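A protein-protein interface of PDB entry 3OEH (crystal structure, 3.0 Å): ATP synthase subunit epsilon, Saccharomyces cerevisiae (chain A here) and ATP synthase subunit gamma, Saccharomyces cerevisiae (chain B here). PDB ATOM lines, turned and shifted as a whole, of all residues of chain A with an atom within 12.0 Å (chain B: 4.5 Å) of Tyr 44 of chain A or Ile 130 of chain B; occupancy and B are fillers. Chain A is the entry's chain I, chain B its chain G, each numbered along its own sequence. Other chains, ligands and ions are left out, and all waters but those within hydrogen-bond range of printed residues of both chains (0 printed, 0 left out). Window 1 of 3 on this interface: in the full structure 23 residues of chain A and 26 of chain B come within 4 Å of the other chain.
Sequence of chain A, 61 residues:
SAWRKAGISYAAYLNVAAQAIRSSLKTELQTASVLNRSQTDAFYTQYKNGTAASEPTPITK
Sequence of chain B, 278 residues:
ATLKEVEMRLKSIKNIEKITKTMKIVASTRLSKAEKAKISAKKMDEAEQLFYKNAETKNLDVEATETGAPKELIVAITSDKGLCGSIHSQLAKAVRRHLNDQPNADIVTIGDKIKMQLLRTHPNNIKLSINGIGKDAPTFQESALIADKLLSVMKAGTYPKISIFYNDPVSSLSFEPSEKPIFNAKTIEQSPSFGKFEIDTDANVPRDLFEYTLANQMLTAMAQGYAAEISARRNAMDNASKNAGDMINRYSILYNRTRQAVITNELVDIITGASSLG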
ATOM      1  N   ILE A   8      27.328  21.580 -32.338  1.00  0.00           N
ATOM      2  CA  ILE A   8      27.779  22.435 -33.469  1.00  0.00           C
ATOM      3  C   ILE A   8      27.056  23.785 -33.451  1.00  0.00           C
ATOM      4  O   ILE A   8      25.819  23.840 -33.484  1.00  0.00           O
ATOM      5  CB  ILE A   8      27.564  21.739 -34.827  1.00  0.00           C
ATOM      6  N   ALA A  12      31.259  27.059 -30.922  1.00  0.00           N
ATOM      7  CA  ALA A  12      31.758  25.688 -30.820  1.00  0.00           C
ATOM      8  C   ALA A  12      32.423  25.222 -32.115  1.00  0.00           C
ATOM      9  O   ALA A  12      33.259  24.318 -32.099  1.00  0.00           O
ATOM     10  CB  ALA A  12      30.618  24.745 -30.441  1.00  0.00           C
ATOM     11  N   GLN A  39      42.417  22.553 -22.381  1.00  0.00           N
ATOM     12  CA  GLN A  39      41.834  21.723 -21.323  1.00  0.00           C
ATOM     13  C   GLN A  39      40.736  22.447 -20.546  1.00  0.00           C
ATOM     14  O   GLN A  39      40.880  23.620 -20.195  1.00  0.00           O
ATOM     15  CB  GLN A  39      42.928  21.223 -20.368  1.00  0.00           C
ATOM     16  N   THR A  40      39.644  21.739 -20.279  1.00  0.00           N
ATOM     17  CA  THR A  40      38.535  22.302 -19.511  1.00  0.00           C
ATOM     18  C   THR A  40      38.058  21.360 -18.404  1.00  0.00           C
ATOM     19  O   THR A  40      37.625  20.234 -18.671  1.00  0.00           O
ATOM     20  CB  THR A  40      37.338  22.693 -20.414  1.00  0.00           C
ATOM     21  N   ASP A  41      38.156  21.833 -17.163  1.00  0.00           N
ATOM     22  CA  ASP A  41      37.572  21.149 -16.012  1.00  0.00           C
ATOM     23  C   ASP A  41      36.159  21.686 -15.780  1.00  0.00           C
ATOM     24  O   ASP A  41      35.828  22.127 -14.682  1.00  0.00           O
ATOM     25  CB  ASP A  41      38.436  21.364 -14.760  1.00  0.00           C
ATOM     26  CG  ASP A  41      39.866  20.876 -14.935  1.00  0.00           C
ATOM     27  OD1 ASP A  41      40.095  19.952 -15.745  1.00  0.00           O
ATOM     28  OD2 ASP A  41      40.762  21.415 -14.248  1.00  0.00           O
ATOM     29  N   ALA A  42      35.329  21.653 -16.819  1.00  0.00           N
ATOM     30  CA  ALA A  42      34.007  22.275 -16.763  1.00  0.00           C
ATOM     31  C   ALA A  42      32.884  21.246 -16.874  1.00  0.00           C
ATOM     32  O   ALA A  42      32.826  20.483 -17.841  1.00  0.00           O
ATOM     33  CB  ALA A  42      33.881  23.331 -17.853  1.00  0.00           C
ATOM     34  N   PHE A  43      31.995  21.231 -15.883  1.00  0.00           N
ATOM     35  CA  PHE A  43      30.895  20.264 -15.844  1.00  0.00           C
ATOM     36  C   PHE A  43      29.534  20.957 -15.719  1.00  0.00           C
ATOM     37  O   PHE A  43      29.243  21.606 -14.710  1.00  0.00           O
ATOM     38  CB  PHE A  43      31.097  19.245 -14.707  1.00  0.00           C
ATOM     39  CG  PHE A  43      32.374  18.447 -14.820  1.00  0.00           C
ATOM     40  CD1 PHE A  43      33.521  18.842 -14.137  1.00  0.00           C
ATOM     41  CD2 PHE A  43      32.429  17.301 -15.611  1.00  0.00           C
ATOM     42  CE1 PHE A  43      34.703  18.113 -14.243  1.00  0.00           C
ATOM     43  CE2 PHE A  43      33.606  16.565 -15.724  1.00  0.00           C
ATOM     44  CZ  PHE A  43      34.745  16.972 -15.037  1.00  0.00           C
ATOM     45  N   TYR A  44      28.698  20.818 -16.743  1.00  0.00           N
ATOM     46  CA  TYR A  44      27.406  21.493 -16.731  1.00  0.00           C
ATOM     47  C   TYR A  44      26.314  20.681 -16.047  1.00  0.00           C
ATOM     48  O   TYR A  44      26.050  19.533 -16.406  1.00  0.00           O
ATOM     49  CB  TYR A  44      27.004  21.994 -18.132  1.00  0.00           C
ATOM     50  CG  TYR A  44      26.514  20.941 -19.089  1.00  0.00           C
ATOM     51  CD1 TYR A  44      27.410  20.122 -19.770  1.00  0.00           C
ATOM     52  CD2 TYR A  44      25.150  20.781 -19.333  1.00  0.00           C
ATOM     53  CE1 TYR A  44      26.957  19.151 -20.657  1.00  0.00           C
ATOM     54  CE2 TYR A  44      24.688  19.817 -20.218  1.00  0.00           C
ATOM     55  CZ  TYR A  44      25.595  19.007 -20.874  1.00  0.00           C
ATOM     56  OH  TYR A  44      25.139  18.053 -21.749  1.00  0.00           O
ATOM     57  N   THR A  45      25.704  21.292 -15.040  1.00  0.00           N
ATOM     58  CA  THR A  45      24.615  20.682 -14.299  1.00  0.00           C
ATOM     59  C   THR A  45      23.316  21.408 -14.610  1.00  0.00           C
ATOM     60  O   THR A  45      23.189  22.609 -14.375  1.00  0.00           O
ATOM     61  CB  THR A  45      24.874  20.719 -12.776  1.00  0.00           C
ATOM     62  OG1 THR A  45      26.126  20.085 -12.485  1.00  0.00           O
ATOM     63  CG2 THR A  45      23.764  20.000 -12.016  1.00  0.00           C
ATOM     64  N   GLN A  46      22.360  20.661 -15.148  1.00  0.00           N
ATOM     65  CA  GLN A  46      21.014  21.162 -15.369  1.00  0.00           C
ATOM     66  C   GLN A  46      20.271  21.249 -14.030  1.00  0.00           C
ATOM     67  O   GLN A  46      20.560  20.496 -13.099  1.00  0.00           O
ATOM     68  CB  GLN A  46      20.295  20.239 -16.347  1.00  0.00           C
ATOM     69  CG  GLN A  46      19.157  20.881 -17.099  1.00  0.00           C
ATOM     70  CD  GLN A  46      19.112  20.467 -18.555  1.00  0.00           C
ATOM     71  OE1 GLN A  46      19.981  19.739 -19.042  1.00  0.00           O
ATOM     72  NE2 GLN A  46      18.099  20.943 -19.264  1.00  0.00           N
ATOM     73  N   TYR A  47      19.324  22.176 -13.935  1.00  0.00           N
ATOM     74  CA  TYR A  47      18.641  22.457 -12.673  1.00  0.00           C
ATOM     75  C   TYR A  47      17.146  22.723 -12.885  1.00  0.00           C
ATOM     76  O   TYR A  47      16.762  23.381 -13.859  1.00  0.00           O
ATOM     77  CB  TYR A  47      19.307  23.656 -11.988  1.00  0.00           C
ATOM     78  CG  TYR A  47      20.179  23.332 -10.783  1.00  0.00           C
ATOM     79  CD1 TYR A  47      21.416  22.697 -10.926  1.00  0.00           C
ATOM     80  CD2 TYR A  47      19.774  23.700  -9.498  1.00  0.00           C
ATOM     81  CE1 TYR A  47      22.213  22.421  -9.815  1.00  0.00           C
ATOM     82  CE2 TYR A  47      20.560  23.428  -8.387  1.00  0.00           C
ATOM     83  CZ  TYR A  47      21.776  22.790  -8.549  1.00  0.00           C
ATOM     84  OH  TYR A  47      22.545  22.522  -7.434  1.00  0.00           O
ATOM     85  N   LYS A  48      16.314  22.207 -11.974  1.00  0.00           N
ATOM     86  CA  LYS A  48      14.847  22.334 -12.073  1.00  0.00           C
ATOM     87  C   LYS A  48      14.130  22.361 -10.723  1.00  0.00           C
ATOM     88  O   LYS A  48      14.364  21.508  -9.864  1.00  0.00           O
ATOM     89  CB  LYS A  48      14.246  21.226 -12.953  1.00  0.00           C
ATOM     90  N   SER A  54      18.270  21.025  -7.392  1.00  0.00           N
ATOM     91  CA  SER A  54      18.758  20.353  -8.606  1.00  0.00           C
ATOM     92  C   SER A  54      17.802  19.360  -9.259  1.00  0.00           C
ATOM     93  O   SER A  54      16.796  18.962  -8.665  1.00  0.00           O
ATOM     94  CB  SER A  54      20.084  19.643  -8.320  1.00  0.00           C
ATOM     95  OG  SER A  54      20.557  18.973  -9.479  1.00  0.00           O
ATOM     96  N   GLU A  55      18.153  18.960 -10.485  1.00  0.00           N
ATOM     97  CA  GLU A  55      17.376  17.990 -11.257  1.00  0.00           C
ATOM     98  C   GLU A  55      18.201  16.790 -11.790  1.00  0.00           C
ATOM     99  O   GLU A  55      18.176  15.719 -11.170  1.00  0.00           O
ATOM    100  CB  GLU A  55      16.575  18.687 -12.365  1.00  0.00           C
ATOM    101  N   PRO A  56      18.917  16.944 -12.935  1.00  0.00           N
ATOM    102  CA  PRO A  56      19.634  15.783 -13.477  1.00  0.00           C
ATOM    103  C   PRO A  56      21.167  15.767 -13.305  1.00  0.00           C
ATOM    104  O   PRO A  56      21.745  16.670 -12.686  1.00  0.00           O
ATOM    105  CB  PRO A  56      19.270  15.820 -14.973  1.00  0.00           C
ATOM    106  CG  PRO A  56      18.645  17.189 -15.215  1.00  0.00           C
ATOM    107  CD  PRO A  56      18.806  17.991 -13.958  1.00  0.00           C
ATOM    108  N   THR A  57      21.793  14.731 -13.870  1.00  0.00           N
ATOM    109  CA  THR A  57      23.231  14.443 -13.738  1.00  0.00           C
ATOM    110  C   THR A  57      24.177  15.500 -14.341  1.00  0.00           C
ATOM    111  O   THR A  57      23.886  16.064 -15.401  1.00  0.00           O
ATOM    112  CB  THR A  57      23.577  13.014 -14.295  1.00  0.00           C
ATOM    113  OG1 THR A  57      24.835  13.042 -14.984  1.00  0.00           O
ATOM    114  CG2 THR A  57      22.501  12.508 -15.257  1.00  0.00           C
ATOM    115  N   PRO A  58      25.311  15.778 -13.650  1.00  0.00           N
ATOM    116  CA  PRO A  58      26.368  16.680 -14.140  1.00  0.00           C
ATOM    117  C   PRO A  58      27.264  16.053 -15.216  1.00  0.00           C
ATOM    118  O   PRO A  58      27.965  15.076 -14.946  1.00  0.00           O
ATOM    119  CB  PRO A  58      27.188  16.983 -12.878  1.00  0.00           C
ATOM    120  CG  PRO A  58      26.956  15.825 -11.984  1.00  0.00           C
ATOM    121  CD  PRO A  58      25.553  15.364 -12.252  1.00  0.00           C
ATOM    122  N   ILE A  59      27.245  16.623 -16.419  1.00  0.00           N
ATOM    123  CA  ILE A  59      28.009  16.089 -17.545  1.00  0.00           C
ATOM    124  C   ILE A  59      29.211  16.959 -17.903  1.00  0.00           C
ATOM    125  O   ILE A  59      29.192  18.171 -17.694  1.00  0.00           O
ATOM    126  CB  ILE A  59      27.122  15.936 -18.796  1.00  0.00           C
ATOM    127  N   THR A  60      30.253  16.329 -18.444  1.00  0.00           N
ATOM    128  CA  THR A  60      31.411  17.049 -18.974  1.00  0.00           C
ATOM    129  C   THR A  60      30.990  17.981 -20.125  1.00  0.00           C
ATOM    130  O   THR A  60      30.025  17.690 -20.841  1.00  0.00           O
ATOM    131  CB  THR A  60      32.511  16.074 -19.442  1.00  0.00           C
ATOM    132  N   LYS A  61      31.704  19.096 -20.288  1.00  0.00           N
ATOM    133  CA  LYS A  61      31.345  20.124 -21.279  1.00  0.00           C
ATOM    134  C   LYS A  61      31.570  19.671 -22.726  1.00  0.00           C
ATOM    135  O   LYS A  61      32.215  18.652 -22.990  1.00  0.00           O
ATOM    136  CB  LYS A  61      32.098  21.432 -21.001  1.00  0.00           C
ATOM    137  N   ASP B  80      33.931  29.170  -8.401  1.00  0.00           N
ATOM    138  CA  ASP B  80      33.725  28.031  -7.517  1.00  0.00           C
ATOM    139  C   ASP B  80      34.404  28.238  -6.165  1.00  0.00           C
ATOM    140  O   ASP B  80      33.961  27.699  -5.151  1.00  0.00           O
ATOM    141  CB  ASP B  80      34.301  26.776  -8.169  1.00  0.00           C
ATOM    142  CG  ASP B  80      33.274  25.990  -8.966  1.00  0.00           C
ATOM    143  OD1 ASP B  80      32.262  26.557  -9.435  1.00  0.00           O
ATOM    144  OD2 ASP B  80      33.493  24.772  -9.123  1.00  0.00           O
ATOM    145  N   THR B 109      23.920  30.017 -13.892  1.00  0.00           N
ATOM    146  CA  THR B 109      25.039  30.329 -13.023  1.00  0.00           C
ATOM    147  C   THR B 109      26.318  29.689 -13.525  1.00  0.00           C
ATOM    148  O   THR B 109      26.337  28.529 -13.949  1.00  0.00           O
ATOM    149  CB  THR B 109      24.794  29.853 -11.585  1.00  0.00           C
ATOM    150  OG1 THR B 109      24.425  28.469 -11.602  1.00  0.00           O
ATOM    151  CG2 THR B 109      23.684  30.670 -10.923  1.00  0.00           C
ATOM    152  N   ILE B 110      27.384  30.475 -13.483  1.00  0.00           N
ATOM    153  CA  ILE B 110      28.716  29.990 -13.751  1.00  0.00           C
ATOM    154  C   ILE B 110      29.484  30.198 -12.456  1.00  0.00           C
ATOM    155  O   ILE B 110      29.662  31.336 -12.013  1.00  0.00           O
ATOM    156  CB  ILE B 110      29.351  30.748 -14.933  1.00  0.00           C
ATOM    157  CG1 ILE B 110      28.493  30.558 -16.188  1.00  0.00           C
ATOM    158  CG2 ILE B 110      30.784  30.277 -15.170  1.00  0.00           C
ATOM    159  CD1 ILE B 110      29.019  31.241 -17.415  1.00  0.00           C
ATOM    160  N   GLY B 111      29.906  29.092 -11.841  1.00  0.00           N
ATOM    161  CA  GLY B 111      30.537  29.111 -10.517  1.00  0.00           C
ATOM    162  C   GLY B 111      29.575  28.738  -9.396  1.00  0.00           C
ATOM    163  O   GLY B 111      28.452  29.224  -9.352  1.00  0.00           O
ATOM    164  N   ASP B 112      30.014  27.878  -8.484  1.00  0.00           N
ATOM    165  CA  ASP B 112      29.146  27.403  -7.399  1.00  0.00           C
ATOM    166  C   ASP B 112      28.838  28.430  -6.303  1.00  0.00           C
ATOM    167  O   ASP B 112      27.720  28.453  -5.786  1.00  0.00           O
ATOM    168  CB  ASP B 112      29.692  26.115  -6.779  1.00  0.00           C
ATOM    169  CG  ASP B 112      29.277  24.870  -7.546  1.00  0.00           C
ATOM    170  OD1 ASP B 112      28.242  24.905  -8.244  1.00  0.00           O
ATOM    171  OD2 ASP B 112      29.984  23.845  -7.444  1.00  0.00           O
ATOM    172  N   LEU B 128      20.305  26.321 -15.051  1.00  0.00           N
ATOM    173  CA  LEU B 128      21.609  25.736 -15.376  1.00  0.00           C
ATOM    174  C   LEU B 128      22.700  26.247 -14.434  1.00  0.00           C
ATOM    175  O   LEU B 128      22.648  27.392 -13.971  1.00  0.00           O
ATOM    176  CB  LEU B 128      21.998  26.012 -16.839  1.00  0.00           C
ATOM    177  CG  LEU B 128      23.034  25.095 -17.507  1.00  0.00           C
ATOM    178  CD1 LEU B 128      22.452  23.718 -17.807  1.00  0.00           C
ATOM    179  CD2 LEU B 128      23.564  25.715 -18.779  1.00  0.00           C
ATOM    180  N   SER B 129      23.674  25.382 -14.150  1.00  0.00           N
ATOM    181  CA  SER B 129      24.860  25.752 -13.388  1.00  0.00           C
ATOM    182  C   SER B 129      26.130  25.261 -14.074  1.00  0.00           C
ATOM    183  O   SER B 129      26.171  24.154 -14.608  1.00  0.00           O
ATOM    184  CB  SER B 129      24.789  25.192 -11.970  1.00  0.00           C
ATOM    185  OG  SER B 129      25.880  25.659 -11.187  1.00  0.00           O
ATOM    186  N   ILE B 130      27.166  26.091 -14.050  1.00  0.00           N
ATOM    187  CA  ILE B 130      28.464  25.696 -14.581  1.00  0.00           C
ATOM    188  C   ILE B 130      29.457  25.468 -13.432  1.00  0.00           C
ATOM    189  O   ILE B 130      29.535  26.281 -12.510  1.00  0.00           O
ATOM    190  CB  ILE B 130      28.986  26.714 -15.634  1.00  0.00           C
ATOM    191  CG1 ILE B 130      27.968  26.894 -16.771  1.00  0.00           C
ATOM    192  CG2 ILE B 130      30.331  26.289 -16.191  1.00  0.00           C
ATOM    193  CD1 ILE B 130      27.585  25.615 -17.519  1.00  0.00           C
ATOM    194  N   ASN B 131      30.194  24.353 -13.504  1.00  0.00           N
ATOM    195  CA  ASN B 131      31.103  23.884 -12.441  1.00  0.00           C
ATOM    196  C   ASN B 131      32.581  23.949 -12.793  1.00  0.00           C
ATOM    197  O   ASN B 131      32.950  23.894 -13.966  1.00  0.00           O
ATOM    198  CB  ASN B 131      30.782  22.431 -12.077  1.00  0.00           C
ATOM    199  CG  ASN B 131      30.027  22.302 -10.778  1.00  0.00           C
ATOM    200  OD1 ASN B 131      29.402  23.247 -10.307  1.00  0.00           O
ATOM    201  ND2 ASN B 131      30.076  21.117 -10.190  1.00  0.00           N
ATOM    202  N   ILE B 133      35.370  26.330 -12.224  1.00  0.00           N
ATOM    203  CA  ILE B 133      35.432  27.502 -13.077  1.00  0.00           C
ATOM    204  C   ILE B 133      36.556  28.511 -12.861  1.00  0.00           C
ATOM    205  O   ILE B 133      36.960  29.178 -13.818  1.00  0.00           O
ATOM    206  CB  ILE B 133      34.032  28.170 -13.184  1.00  0.00           C
ATOM    207  CG1 ILE B 133      33.358  27.719 -14.484  1.00  0.00           C
ATOM    208  CG2 ILE B 133      34.092  29.707 -13.073  1.00  0.00           C
ATOM    209  CD1 ILE B 133      34.318  27.533 -15.674  1.00  0.00           C
ATOM    210  N   ILE B 146      30.414  26.809 -22.870  1.00  0.00           N
ATOM    211  CA  ILE B 146      29.336  27.278 -22.010  1.00  0.00           C
ATOM    212  C   ILE B 146      28.294  27.911 -22.919  1.00  0.00           C
ATOM    213  O   ILE B 146      27.099  27.653 -22.767  1.00  0.00           O
ATOM    214  CB  ILE B 146      29.800  28.307 -20.945  1.00  0.00           C
ATOM    215  CG1 ILE B 146      30.714  27.654 -19.901  1.00  0.00           C
ATOM    216  CG2 ILE B 146      28.587  28.939 -20.249  1.00  0.00           C
ATOM    217  CD1 ILE B 146      31.463  28.651 -19.036  1.00  0.00           C
ATOM    218  N   LYS B 149      26.124  25.281 -24.854  1.00  0.00           N
ATOM    219  CA  LYS B 149      25.062  24.672 -24.070  1.00  0.00           C
ATOM    220  C   LYS B 149      23.939  25.686 -23.874  1.00  0.00           C
ATOM    221  O   LYS B 149      22.760  25.336 -23.949  1.00  0.00           O
ATOM    222  CB  LYS B 149      25.595  24.159 -22.730  1.00  0.00           C
ATOM    223  CG  LYS B 149      26.748  23.160 -22.849  1.00  0.00           C
ATOM    224  CD  LYS B 149      26.289  21.800 -23.373  1.00  0.00           C
ATOM    225  CE  LYS B 149      27.466  20.949 -23.844  1.00  0.00           C
ATOM    226  NZ  LYS B 149      28.149  21.534 -25.044  1.00  0.00           N
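The backbone NH (N) of Ser 129 of chain B lies within hydrogen-bond range of the backbone carbonyl oxygen (O) of Thr 45 of chain A.
O of Asn 131 of chain B lies close to O of Asp 41 of chain A (3.5 Å).
The backbone NH of Asn 131 of chain B lies within hydrogen-bond range of the backbone carbonyl oxygen of Phe 43 of chain A (3.1 Å).
OG1 of Thr 109 of chain B is in hydrogen-bond range of OG of Ser 129 of chain B (3.2 Å).
The backbone carbonyl oxygen (O) of Leu 128 of chain B lies within hydrogen-bond range of the backbone NH (N) of Thr 109 of chain B (2.9 Å).
O of Thr 109 of chain B is in hydrogen-bond range of N of Ile 130 of chain B (2.6 Å).
The backbone NH (N) of Gly 111 of chain B is in hydrogen-bond range of the backbone carbonyl oxygen (O) of Ile 130 of chain B, at 2.9 Å.
O of Ile 59 of chain A lies within hydrogen-bond range of N of Tyr 44 of chain A (2.9 Å).
O of Ala 42 of chain A sits at hydrogen-bond distance from N of Lys 61 of chain A, at 3.0 Å.
Among the printed residues, pairs that only touch across the chains: Ala 42 of chain A with Asn 131 of chain B (3.4 Å), Phe 43 of chain A with Ser 129 of chain B (3.99 Å), Tyr 44 of chain A with Ser 129 of chain B (3.6 Å), Tyr 44 of chain A with Ile 130 of chain B (3.7 Å), Tyr 44 of chain A with Lys 149 of chain B (3.7 Å), Thr 45 of chain A with Leu 128 of chain B (3.6 Å) and Gln 46 of chain A with Leu 128 of chain B (3.8 Å).
Tyr 44 of chain A touches three residues of chain B.
Ile 130 of chain B touches one residue of chain A.
No residue of chain A comes within 4 Å of Thr 109 of chain B.
Ile 110 of chain B touches none of the printed residues of chain A.
No residue of chain A comes within 4 Å of Asp 112 of chain B.
Leu 128 of chain B touches just these residues of chain A: Thr 45 and Gln 46.
Of chain A, only Asp 41, Ala 42 and Phe 43 come within 4 Å of Asn 131 of chain B.
No residue of chain A comes within 4 Å of Ile 133 of chain B.
Printed residues of chain B within 4 Å of Ala 42 of chain A: Asn 131 (3.4 Å).
Of the printed residues of chain B, Thr 45 of chain A touches Leu 128 and Ser 129.
Of the printed residues of chain A, Ser 129 of chain B touches Phe 43, Tyr 44 and Thr 45.
Pro 56 of chain A touches none of the printed residues of chain B.
The nearest printed residue of chain B that does not touch Gln 46 of chain A is Ser 129 of chain B (5.0 Å).
Hydrophobic or aromatic side chains of chain B that line the printed part of chain A: Leu 128 and Ile 130.
Printed residues of chain A that touch a printed residue of chain B: Asp 41, Ala 42, Phe 43, Tyr 44, Thr 45 and Gln 46.
Among the printed residues, no Asp or Glu carboxylate lies within 4 Å of a Lys or Arg side-chain nitrogen of the other chain.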
